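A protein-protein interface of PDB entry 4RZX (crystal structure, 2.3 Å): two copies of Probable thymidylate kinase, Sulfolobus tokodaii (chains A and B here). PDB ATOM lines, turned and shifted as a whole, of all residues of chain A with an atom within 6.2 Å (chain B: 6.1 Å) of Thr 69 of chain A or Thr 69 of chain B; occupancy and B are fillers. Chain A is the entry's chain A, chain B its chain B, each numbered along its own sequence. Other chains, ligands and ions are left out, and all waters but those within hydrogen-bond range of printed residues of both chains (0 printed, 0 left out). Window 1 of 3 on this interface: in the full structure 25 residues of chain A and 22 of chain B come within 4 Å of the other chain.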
ATOM      1  N   ILE A  45       2.167   8.869  -8.895  1.00  0.00           N
ATOM      2  CA  ILE A  45       2.081   8.656 -10.312  1.00  0.00           C
ATOM      3  C   ILE A  45       1.340   9.840 -10.920  1.00  0.00           C
ATOM      4  O   ILE A  45       1.709  10.379 -11.917  1.00  0.00           O
ATOM      5  CB  ILE A  45       1.316   7.329 -10.645  1.00  0.00           C
ATOM      6  CG1 ILE A  45       2.137   6.135 -10.274  1.00  0.00           C
ATOM      7  CG2 ILE A  45       1.016   7.216 -12.127  1.00  0.00           C
ATOM      8  CD1 ILE A  45       1.372   4.808 -10.426  1.00  0.00           C
ATOM      9  N   ILE A  49       2.938  12.833 -13.564  1.00  0.00           N
ATOM     10  CA  ILE A  49       2.342  13.017 -14.876  1.00  0.00           C
ATOM     11  C   ILE A  49       1.890  14.460 -15.017  1.00  0.00           C
ATOM     12  O   ILE A  49       2.210  15.128 -15.997  1.00  0.00           O
ATOM     13  CB  ILE A  49       1.163  12.053 -15.124  1.00  0.00           C
ATOM     14  CG1 ILE A  49       1.675  10.604 -15.123  1.00  0.00           C
ATOM     15  CG2 ILE A  49       0.573  12.342 -16.481  1.00  0.00           C
ATOM     16  CD1 ILE A  49       0.603   9.534 -15.286  1.00  0.00           C
ATOM     17  N   THR A  62      -7.775  12.363 -20.956  1.00  0.00           N
ATOM     18  CA  THR A  62      -6.438  12.182 -20.407  1.00  0.00           C
ATOM     19  C   THR A  62      -6.440  12.522 -18.893  1.00  0.00           C
ATOM     20  O   THR A  62      -5.905  11.779 -18.087  1.00  0.00           O
ATOM     21  CB  THR A  62      -5.430  13.040 -21.200  1.00  0.00           C
ATOM     22  OG1 THR A  62      -5.356  12.552 -22.532  1.00  0.00           O
ATOM     23  CG2 THR A  62      -4.031  12.933 -20.600  1.00  0.00           C
ATOM     24  N   SER A  64      -8.929  12.314 -16.935  1.00  0.00           N
ATOM     25  CA  SER A  64      -9.616  11.184 -16.350  1.00  0.00           C
ATOM     26  C   SER A  64      -8.751   9.909 -16.209  1.00  0.00           C
ATOM     27  O   SER A  64      -8.805   9.245 -15.188  1.00  0.00           O
ATOM     28  CB  SER A  64     -10.831  10.818 -17.176  1.00  0.00           C
ATOM     29  OG  SER A  64     -11.232   9.502 -16.843  1.00  0.00           O
ATOM     30  N   LEU A  65      -7.910   9.591 -17.202  1.00  0.00           N
ATOM     31  CA  LEU A  65      -7.028   8.420 -17.084  1.00  0.00           C
ATOM     32  C   LEU A  65      -5.895   8.630 -16.095  1.00  0.00           C
ATOM     33  O   LEU A  65      -5.355   7.674 -15.518  1.00  0.00           O
ATOM     34  CB  LEU A  65      -6.498   7.994 -18.443  1.00  0.00           C
ATOM     35  CG  LEU A  65      -7.561   7.321 -19.302  1.00  0.00           C
ATOM     36  CD1 LEU A  65      -7.327   7.522 -20.807  1.00  0.00           C
ATOM     37  CD2 LEU A  65      -7.602   5.852 -18.999  1.00  0.00           C
ATOM     38  N   ILE A  66      -5.506   9.867 -15.879  1.00  0.00           N
ATOM     39  CA  ILE A  66      -4.397  10.108 -14.975  1.00  0.00           C
ATOM     40  C   ILE A  66      -4.901   9.719 -13.586  1.00  0.00           C
ATOM     41  O   ILE A  66      -4.280   8.942 -12.851  1.00  0.00           O
ATOM     42  CB  ILE A  66      -3.987  11.572 -15.045  1.00  0.00           C
ATOM     43  CG1 ILE A  66      -3.186  11.791 -16.335  1.00  0.00           C
ATOM     44  CG2 ILE A  66      -3.112  11.967 -13.875  1.00  0.00           C
ATOM     45  CD1 ILE A  66      -2.950  13.256 -16.635  1.00  0.00           C
ATOM     46  N   HIS A  67      -6.096  10.181 -13.263  1.00  0.00           N
ATOM     47  CA  HIS A  67      -6.678   9.864 -11.974  1.00  0.00           C
ATOM     48  C   HIS A  67      -7.062   8.402 -11.740  1.00  0.00           C
ATOM     49  O   HIS A  67      -6.823   7.860 -10.645  1.00  0.00           O
ATOM     50  CB  HIS A  67      -7.809  10.807 -11.712  1.00  0.00           C
ATOM     51  CG  HIS A  67      -7.339  12.219 -11.560  1.00  0.00           C
ATOM     52  ND1 HIS A  67      -7.222  13.085 -12.626  1.00  0.00           N
ATOM     53  CD2 HIS A  67      -6.918  12.906 -10.468  1.00  0.00           C
ATOM     54  CE1 HIS A  67      -6.779  14.252 -12.195  1.00  0.00           C
ATOM     55  NE2 HIS A  67      -6.608  14.180 -10.885  1.00  0.00           N
ATOM     56  N   ALA A  68      -7.596   7.748 -12.762  1.00  0.00           N
ATOM     57  CA  ALA A  68      -7.832   6.328 -12.663  1.00  0.00           C
ATOM     58  C   ALA A  68      -6.545   5.529 -12.504  1.00  0.00           C
ATOM     59  O   ALA A  68      -6.503   4.568 -11.719  1.00  0.00           O
ATOM     60  CB  ALA A  68      -8.613   5.855 -13.850  1.00  0.00           C
ATOM     61  N   THR A  69      -5.483   5.950 -13.189  1.00  0.00           N
ATOM     62  CA  THR A  69      -4.227   5.253 -13.100  1.00  0.00           C
ATOM     63  C   THR A  69      -3.695   5.321 -11.682  1.00  0.00           C
ATOM     64  O   THR A  69      -3.363   4.316 -11.067  1.00  0.00           O
ATOM     65  CB  THR A  69      -3.176   5.864 -14.032  1.00  0.00           C
ATOM     66  OG1 THR A  69      -3.594   5.701 -15.378  1.00  0.00           O
ATOM     67  CG2 THR A  69      -1.844   5.166 -13.863  1.00  0.00           C
ATOM     68  N   ASP A  70      -3.619   6.537 -11.169  1.00  0.00           N
ATOM     69  CA  ASP A  70      -3.199   6.760  -9.801  1.00  0.00           C
ATOM     70  C   ASP A  70      -4.108   6.030  -8.847  1.00  0.00           C
ATOM     71  O   ASP A  70      -3.616   5.354  -7.942  1.00  0.00           O
ATOM     72  CB  ASP A  70      -3.179   8.257  -9.499  1.00  0.00           C
ATOM     73  CG  ASP A  70      -2.538   8.600  -8.152  1.00  0.00           C
ATOM     74  OD1 ASP A  70      -1.280   8.720  -8.091  1.00  0.00           O
ATOM     75  OD2 ASP A  70      -3.307   8.847  -7.191  1.00  0.00           O
ATOM     76  N   PHE A  71      -5.418   6.077  -9.048  1.00  0.00           N
ATOM     77  CA  PHE A  71      -6.278   5.317  -8.130  1.00  0.00           C
ATOM     78  C   PHE A  71      -6.005   3.802  -8.191  1.00  0.00           C
ATOM     79  O   PHE A  71      -5.981   3.135  -7.146  1.00  0.00           O
ATOM     80  CB  PHE A  71      -7.737   5.577  -8.393  1.00  0.00           C
ATOM     81  CG  PHE A  71      -8.678   4.764  -7.529  1.00  0.00           C
ATOM     82  CD1 PHE A  71      -8.724   4.952  -6.169  1.00  0.00           C
ATOM     83  CD2 PHE A  71      -9.544   3.868  -8.087  1.00  0.00           C
ATOM     84  CE1 PHE A  71      -9.615   4.240  -5.384  1.00  0.00           C
ATOM     85  CE2 PHE A  71     -10.416   3.148  -7.313  1.00  0.00           C
ATOM     86  CZ  PHE A  71     -10.456   3.341  -5.962  1.00  0.00           C
ATOM     87  N   SER A  72      -5.780   3.233  -9.372  1.00  0.00           N
ATOM     88  CA  SER A  72      -5.508   1.769  -9.444  1.00  0.00           C
ATOM     89  C   SER A  72      -4.342   1.320  -8.534  1.00  0.00           C
ATOM     90  O   SER A  72      -4.380   0.222  -7.949  1.00  0.00           O
ATOM     91  CB  SER A  72      -5.274   1.291 -10.876  1.00  0.00           C
ATOM     92  OG  SER A  72      -4.030   1.771 -11.401  1.00  0.00           O
ATOM     93  N   ASP A  73      -3.323   2.166  -8.402  1.00  0.00           N
ATOM     94  CA  ASP A  73      -2.163   1.898  -7.556  1.00  0.00           C
ATOM     95  C   ASP A  73      -2.562   1.964  -6.078  1.00  0.00           C
ATOM     96  O   ASP A  73      -2.270   1.054  -5.284  1.00  0.00           O
ATOM     97  CB  ASP A  73      -1.122   2.953  -7.848  1.00  0.00           C
ATOM     98  CG  ASP A  73       0.152   2.782  -7.057  1.00  0.00           C
ATOM     99  OD1 ASP A  73       0.670   1.662  -7.052  1.00  0.00           O
ATOM    100  OD2 ASP A  73       0.679   3.796  -6.494  1.00  0.00           O
ATOM    101  N   ARG A  74      -3.237   3.041  -5.695  1.00  0.00           N
ATOM    102  CA  ARG A  74      -3.711   3.165  -4.320  1.00  0.00           C
ATOM    103  C   ARG A  74      -4.624   2.043  -3.921  1.00  0.00           C
ATOM    104  O   ARG A  74      -4.518   1.562  -2.816  1.00  0.00           O
ATOM    105  CB  ARG A  74      -4.373   4.521  -4.085  1.00  0.00           C
ATOM    106  CG  ARG A  74      -3.317   5.614  -4.243  1.00  0.00           C
ATOM    107  CD  ARG A  74      -3.727   6.965  -3.737  1.00  0.00           C
ATOM    108  NE  ARG A  74      -4.659   7.597  -4.642  1.00  0.00           N
ATOM    109  CZ  ARG A  74      -5.820   8.120  -4.257  1.00  0.00           C
ATOM    110  NH1 ARG A  74      -6.196   8.089  -2.965  1.00  0.00           N
ATOM    111  NH2 ARG A  74      -6.596   8.709  -5.161  1.00  0.00           N
ATOM    112  N   TYR A 116     -13.450   2.190 -14.358  1.00  0.00           N
ATOM    113  CA  TYR A 116     -13.283   1.871 -12.969  1.00  0.00           C
ATOM    114  C   TYR A 116     -13.833   0.503 -12.542  1.00  0.00           C
ATOM    115  O   TYR A 116     -13.844   0.193 -11.314  1.00  0.00           O
ATOM    116  CB  TYR A 116     -13.945   2.969 -12.121  1.00  0.00           C
ATOM    117  CG  TYR A 116     -13.095   4.171 -12.018  1.00  0.00           C
ATOM    118  CD1 TYR A 116     -12.076   4.207 -11.102  1.00  0.00           C
ATOM    119  CD2 TYR A 116     -13.264   5.278 -12.885  1.00  0.00           C
ATOM    120  CE1 TYR A 116     -11.258   5.294 -11.013  1.00  0.00           C
ATOM    121  CE2 TYR A 116     -12.449   6.419 -12.781  1.00  0.00           C
ATOM    122  CZ  TYR A 116     -11.462   6.424 -11.838  1.00  0.00           C
ATOM    123  OH  TYR A 116     -10.565   7.471 -11.695  1.00  0.00           O
ATOM    124  N   TRP B  44       7.372  11.540 -19.759  1.00  0.00           N
ATOM    125  CA  TRP B  44       7.184  11.108 -18.368  1.00  0.00           C
ATOM    126  C   TRP B  44       7.067   9.620 -18.046  1.00  0.00           C
ATOM    127  O   TRP B  44       7.288   9.211 -16.900  1.00  0.00           O
ATOM    128  CB  TRP B  44       5.894  11.721 -17.888  1.00  0.00           C
ATOM    129  CG  TRP B  44       4.676  11.453 -18.734  1.00  0.00           C
ATOM    130  CD1 TRP B  44       4.195  12.234 -19.735  1.00  0.00           C
ATOM    131  CD2 TRP B  44       3.750  10.366 -18.598  1.00  0.00           C
ATOM    132  NE1 TRP B  44       3.039  11.698 -20.240  1.00  0.00           N
ATOM    133  CE2 TRP B  44       2.746  10.551 -19.560  1.00  0.00           C
ATOM    134  CE3 TRP B  44       3.680   9.256 -17.763  1.00  0.00           C
ATOM    135  CZ2 TRP B  44       1.679   9.668 -19.709  1.00  0.00           C
ATOM    136  CZ3 TRP B  44       2.626   8.377 -17.909  1.00  0.00           C
ATOM    137  CH2 TRP B  44       1.641   8.579 -18.892  1.00  0.00           C
ATOM    138  N   THR B  62      -2.256  -1.344 -13.395  1.00  0.00           N
ATOM    139  CA  THR B  62      -1.746   0.010 -13.381  1.00  0.00           C
ATOM    140  C   THR B  62      -0.858   0.283 -14.617  1.00  0.00           C
ATOM    141  O   THR B  62      -0.881   1.392 -15.211  1.00  0.00           O
ATOM    142  CB  THR B  62      -0.979   0.304 -12.097  1.00  0.00           C
ATOM    143  OG1 THR B  62      -1.854   0.169 -10.969  1.00  0.00           O
ATOM    144  CG2 THR B  62      -0.407   1.787 -12.138  1.00  0.00           C
ATOM    145  N   SER B  64      -1.115  -0.979 -17.613  1.00  0.00           N
ATOM    146  CA  SER B  64      -2.056  -0.820 -18.705  1.00  0.00           C
ATOM    147  C   SER B  64      -2.670   0.590 -18.700  1.00  0.00           C
ATOM    148  O   SER B  64      -2.847   1.216 -19.755  1.00  0.00           O
ATOM    149  CB  SER B  64      -3.144  -1.895 -18.563  1.00  0.00           C
ATOM    150  OG  SER B  64      -4.237  -1.705 -19.446  1.00  0.00           O
ATOM    151  N   LEU B  65      -2.983   1.102 -17.522  1.00  0.00           N
ATOM    152  CA  LEU B  65      -3.536   2.451 -17.402  1.00  0.00           C
ATOM    153  C   LEU B  65      -2.470   3.488 -17.761  1.00  0.00           C
ATOM    154  O   LEU B  65      -2.743   4.469 -18.472  1.00  0.00           O
ATOM    155  CB  LEU B  65      -4.072   2.656 -15.968  1.00  0.00           C
ATOM    156  CG  LEU B  65      -5.340   1.845 -15.733  1.00  0.00           C
ATOM    157  CD1 LEU B  65      -5.950   1.894 -14.348  1.00  0.00           C
ATOM    158  CD2 LEU B  65      -6.368   2.403 -16.710  1.00  0.00           C
ATOM    159  N   ILE B  66      -1.255   3.300 -17.263  1.00  0.00           N
ATOM    160  CA  ILE B  66      -0.168   4.225 -17.615  1.00  0.00           C
ATOM    161  C   ILE B  66      -0.022   4.309 -19.133  1.00  0.00           C
ATOM    162  O   ILE B  66       0.034   5.403 -19.708  1.00  0.00           O
ATOM    163  CB  ILE B  66       1.177   3.790 -17.007  1.00  0.00           C
ATOM    164  CG1 ILE B  66       1.189   3.998 -15.525  1.00  0.00           C
ATOM    165  CG2 ILE B  66       2.328   4.582 -17.560  1.00  0.00           C
ATOM    166  CD1 ILE B  66       2.325   3.244 -14.828  1.00  0.00           C
ATOM    167  N   HIS B  67       0.041   3.181 -19.805  1.00  0.00           N
ATOM    168  CA  HIS B  67       0.236   3.263 -21.252  1.00  0.00           C
ATOM    169  C   HIS B  67      -0.998   3.793 -21.915  1.00  0.00           C
ATOM    170  O   HIS B  67      -0.878   4.435 -22.958  1.00  0.00           O
ATOM    171  CB  HIS B  67       0.593   1.903 -21.859  1.00  0.00           C
ATOM    172  CG  HIS B  67       1.985   1.475 -21.547  1.00  0.00           C
ATOM    173  ND1 HIS B  67       2.269   0.372 -20.775  1.00  0.00           N
ATOM    174  CD2 HIS B  67       3.180   2.026 -21.880  1.00  0.00           C
ATOM    175  CE1 HIS B  67       3.581   0.255 -20.646  1.00  0.00           C
ATOM    176  NE2 HIS B  67       4.158   1.240 -21.313  1.00  0.00           N
ATOM    177  N   ALA B  68      -2.189   3.546 -21.344  1.00  0.00           N
ATOM    178  CA  ALA B  68      -3.389   4.091 -21.992  1.00  0.00           C
ATOM    179  C   ALA B  68      -3.461   5.609 -21.841  1.00  0.00           C
ATOM    180  O   ALA B  68      -3.957   6.311 -22.719  1.00  0.00           O
ATOM    181  CB  ALA B  68      -4.652   3.456 -21.453  1.00  0.00           C
ATOM    182  N   THR B  69      -2.967   6.111 -20.713  1.00  0.00           N
ATOM    183  CA  THR B  69      -2.960   7.559 -20.449  1.00  0.00           C
ATOM    184  C   THR B  69      -2.081   8.241 -21.498  1.00  0.00           C
ATOM    185  O   THR B  69      -2.457   9.261 -22.061  1.00  0.00           O
ATOM    186  CB  THR B  69      -2.484   7.842 -19.006  1.00  0.00           C
ATOM    187  OG1 THR B  69      -3.376   7.178 -18.112  1.00  0.00           O
ATOM    188  CG2 THR B  69      -2.487   9.358 -18.675  1.00  0.00           C
ATOM    189  N   ASP B  70      -0.925   7.662 -21.765  1.00  0.00           N
ATOM    190  CA  ASP B  70      -0.002   8.246 -22.727  1.00  0.00           C
ATOM    191  C   ASP B  70      -0.588   8.135 -24.114  1.00  0.00           C
ATOM    192  O   ASP B  70      -0.582   9.109 -24.863  1.00  0.00           O
ATOM    193  CB  ASP B  70       1.304   7.509 -22.674  1.00  0.00           C
ATOM    194  CG  ASP B  70       2.407   8.167 -23.504  1.00  0.00           C
ATOM    195  OD1 ASP B  70       2.436   9.390 -23.726  1.00  0.00           O
ATOM    196  OD2 ASP B  70       3.291   7.419 -23.888  1.00  0.00           O
ATOM    197  N   PHE B  71      -1.191   6.977 -24.418  1.00  0.00           N
ATOM    198  CA  PHE B  71      -1.829   6.817 -25.681  1.00  0.00           C
ATOM    199  C   PHE B  71      -2.934   7.855 -25.877  1.00  0.00           C
ATOM    200  O   PHE B  71      -3.057   8.423 -26.971  1.00  0.00           O
ATOM    201  CB  PHE B  71      -2.440   5.436 -25.829  1.00  0.00           C
ATOM    202  CG  PHE B  71      -3.140   5.267 -27.125  1.00  0.00           C
ATOM    203  CD1 PHE B  71      -2.443   4.932 -28.253  1.00  0.00           C
ATOM    204  CD2 PHE B  71      -4.467   5.533 -27.231  1.00  0.00           C
ATOM    205  CE1 PHE B  71      -3.074   4.863 -29.478  1.00  0.00           C
ATOM    206  CE2 PHE B  71      -5.110   5.433 -28.436  1.00  0.00           C
ATOM    207  CZ  PHE B  71      -4.412   5.120 -29.560  1.00  0.00           C
ATOM    208  N   SER B  72      -3.778   8.061 -24.861  1.00  0.00           N
ATOM    209  CA  SER B  72      -4.863   9.028 -25.004  1.00  0.00           C
ATOM    210  C   SER B  72      -4.343  10.400 -25.298  1.00  0.00           C
ATOM    211  O   SER B  72      -4.976  11.170 -25.997  1.00  0.00           O
ATOM    212  CB  SER B  72      -5.767   9.107 -23.739  1.00  0.00           C
ATOM    213  OG  SER B  72      -5.123   9.673 -22.612  1.00  0.00           O
ATOM    214  N   ASP B  73      -3.201  10.730 -24.722  1.00  0.00           N
ATOM    215  CA  ASP B  73      -2.634  12.066 -24.899  1.00  0.00           C
ATOM    216  C   ASP B  73      -2.211  12.265 -26.345  1.00  0.00           C
ATOM    217  O   ASP B  73      -2.635  13.186 -27.011  1.00  0.00           O
ATOM    218  CB  ASP B  73      -1.443  12.298 -23.959  1.00  0.00           C
ATOM    219  CG  ASP B  73      -0.917  13.697 -24.054  1.00  0.00           C
ATOM    220  OD1 ASP B  73      -1.689  14.624 -23.779  1.00  0.00           O
ATOM    221  OD2 ASP B  73       0.249  13.900 -24.455  1.00  0.00           O
ATOM    222  N   ARG B  74      -1.432  11.348 -26.851  1.00  0.00           N
ATOM    223  CA  ARG B  74      -1.018  11.422 -28.251  1.00  0.00           C
ATOM    224  C   ARG B  74      -2.229  11.324 -29.230  1.00  0.00           C
ATOM    225  O   ARG B  74      -2.262  12.009 -30.277  1.00  0.00           O
ATOM    226  CB  ARG B  74       0.121  10.392 -28.524  1.00  0.00           C
ATOM    227  CG  ARG B  74      -0.274   9.089 -29.188  1.00  0.00           C
ATOM    228  CD  ARG B  74       0.812   8.024 -29.020  1.00  0.00           C
ATOM    229  NE  ARG B  74       0.921   7.124 -30.173  1.00  0.00           N
ATOM    230  CZ  ARG B  74       1.133   5.810 -30.105  1.00  0.00           C
ATOM    231  NH1 ARG B  74       1.234   5.188 -28.928  1.00  0.00           N
ATOM    232  NH2 ARG B  74       1.217   5.100 -31.232  1.00  0.00           N
ATOM    233  N   TYR B 116      -9.779   1.276 -24.526  1.00  0.00           N
ATOM    234  CA  TYR B 116      -9.291   1.933 -25.755  1.00  0.00           C
ATOM    235  C   TYR B 116     -10.395   2.228 -26.728  1.00  0.00           C
ATOM    236  O   TYR B 116     -10.091   2.633 -27.832  1.00  0.00           O
ATOM    237  CB  TYR B 116      -8.194   1.131 -26.447  1.00  0.00           C
ATOM    238  CG  TYR B 116      -6.834   1.278 -25.793  1.00  0.00           C
ATOM    239  CD1 TYR B 116      -5.951   2.298 -26.149  1.00  0.00           C
ATOM    240  CD2 TYR B 116      -6.427   0.386 -24.816  1.00  0.00           C
ATOM    241  CE1 TYR B 116      -4.672   2.417 -25.531  1.00  0.00           C
ATOM    242  CE2 TYR B 116      -5.180   0.493 -24.220  1.00  0.00           C
ATOM    243  CZ  TYR B 116      -4.312   1.496 -24.582  1.00  0.00           C
ATOM    244  OH  TYR B 116      -3.116   1.556 -23.911  1.00  0.00           O
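The side-chain hydroxyl (OG1) of Thr 62 of chain A sits at hydrogen-bond distance from the side-chain hydroxyl (OG) of Ser 72 of chain B, at 2.9 Å. O of Leu 65 of chain B lies close to OG1 of Thr 69 of chain A, at 3.4 Å. The side-chain hydroxyl (OG1) of Thr 69 of chain A lies within hydrogen-bond range of the side-chain hydroxyl (OG1) of Thr 69 of chain B. The side-chain hydroxyl (OG) of Ser 72 of chain A lies within hydrogen-bond range of the side-chain hydroxyl (OG1) of Thr 62 of chain B (2.7 Å). The side-chain hydroxyl (OG1) of Thr 69 of chain B sits close to the backbone carbonyl oxygen (O) of Leu 65 of chain A (3.3 Å).
Printed residues of chain A that touch a printed residue of chain B: Ile 45, Ile 49, Thr 62, Leu 65, Ile 66, Ala 68, Thr 69, Ser 72 and Asp 73. Hydrophobic or aromatic side chains of chain A that line the printed part of chain B: Ile 45, Ile 49, Leu 65 and Ile 66. Among the printed residues, no Asp or Glu carboxylate lies within 4 Å of a Lys or Arg side-chain nitrogen of the other chain.
Thr 69 of chain A touches three residues of chain B. Thr 69 of chain B touches three residues of chain A. Printed residues of chain B within 4 Å of Leu 65 of chain A: Thr 69 and Ser 72. Of the printed residues of chain A, Ile 66 of chain B touches Thr 69 (3.7 Å). The nearest residue of chain B that does not touch Thr 69 of chain A is Thr 62 of chain B (4.03 Å). The nearest residue of chain A that does not touch Thr 69 of chain B is Thr 62 of chain A (4.2 Å). The nearest printed residue of chain B that does not touch Thr 62 of chain A is Thr 69 of chain B (4.2 Å).
Among the printed residues, pairs that only touch across the chains: Ile 45 of chain A with Thr 62 of chain B (3.9 Å), Ile 49 of chain A with Trp 44 of chain B (3.5 Å), Thr 62 of chain A with Asp 73 of chain B (3.6 Å), Leu 65 of chain A with Ser 72 of chain B (3.6 Å), Ile 66 of chain A with Thr 69 of chain B (3.4 Å), Ala 68 of chain A with Leu 65 of chain B (3.8 Å), Thr 69 of chain A with Ile 66 of chain B (3.7 Å), Ser 72 of chain A with Leu 65 of chain B (3.5 Å) and Asp 73 of chain A with Thr 62 of chain B (3.6 Å).
The side-chain hydroxyl (OG) of Ser 72 of chain A is in hydrogen-bond range of the backbone carbonyl oxygen (O) of Thr 69 of chain A (2.7 Å). The side-chain hydroxyl of Thr 69 of chain A lies within hydrogen-bond range of the backbone carbonyl oxygen of Leu 65 of chain A (2.6 Å). OG of Ser 72 of chain B is in hydrogen-bond range of O of Thr 69 of chain B (2.8 Å). The backbone NH (N) of Ala 68 of chain A lies close to the side-chain hydroxyl (OH) of Tyr 116 of chain A, 3.2 Å away. O of Leu 65 of chain B sits at hydrogen-bond distance from OG1 of Thr 69 of chain B (2.8 Å).
Thr 62 of chain A touches Asp 73 of chain B, and with the chains exchanged Asp 73 of chain A touches Thr 62 of chain B. Leu 65 of chain A touches Thr 69 of chain B, and with the chains exchanged Thr 69 of chain A touches Leu 65 of chain B. Ile 66 of chain A touches Thr 69 of chain B, and with the chains exchanged Thr 69 of chain A touches Ile 66 of chain B. Thr 69 of chain B touches its own counterpart, Thr 69 of chain A.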
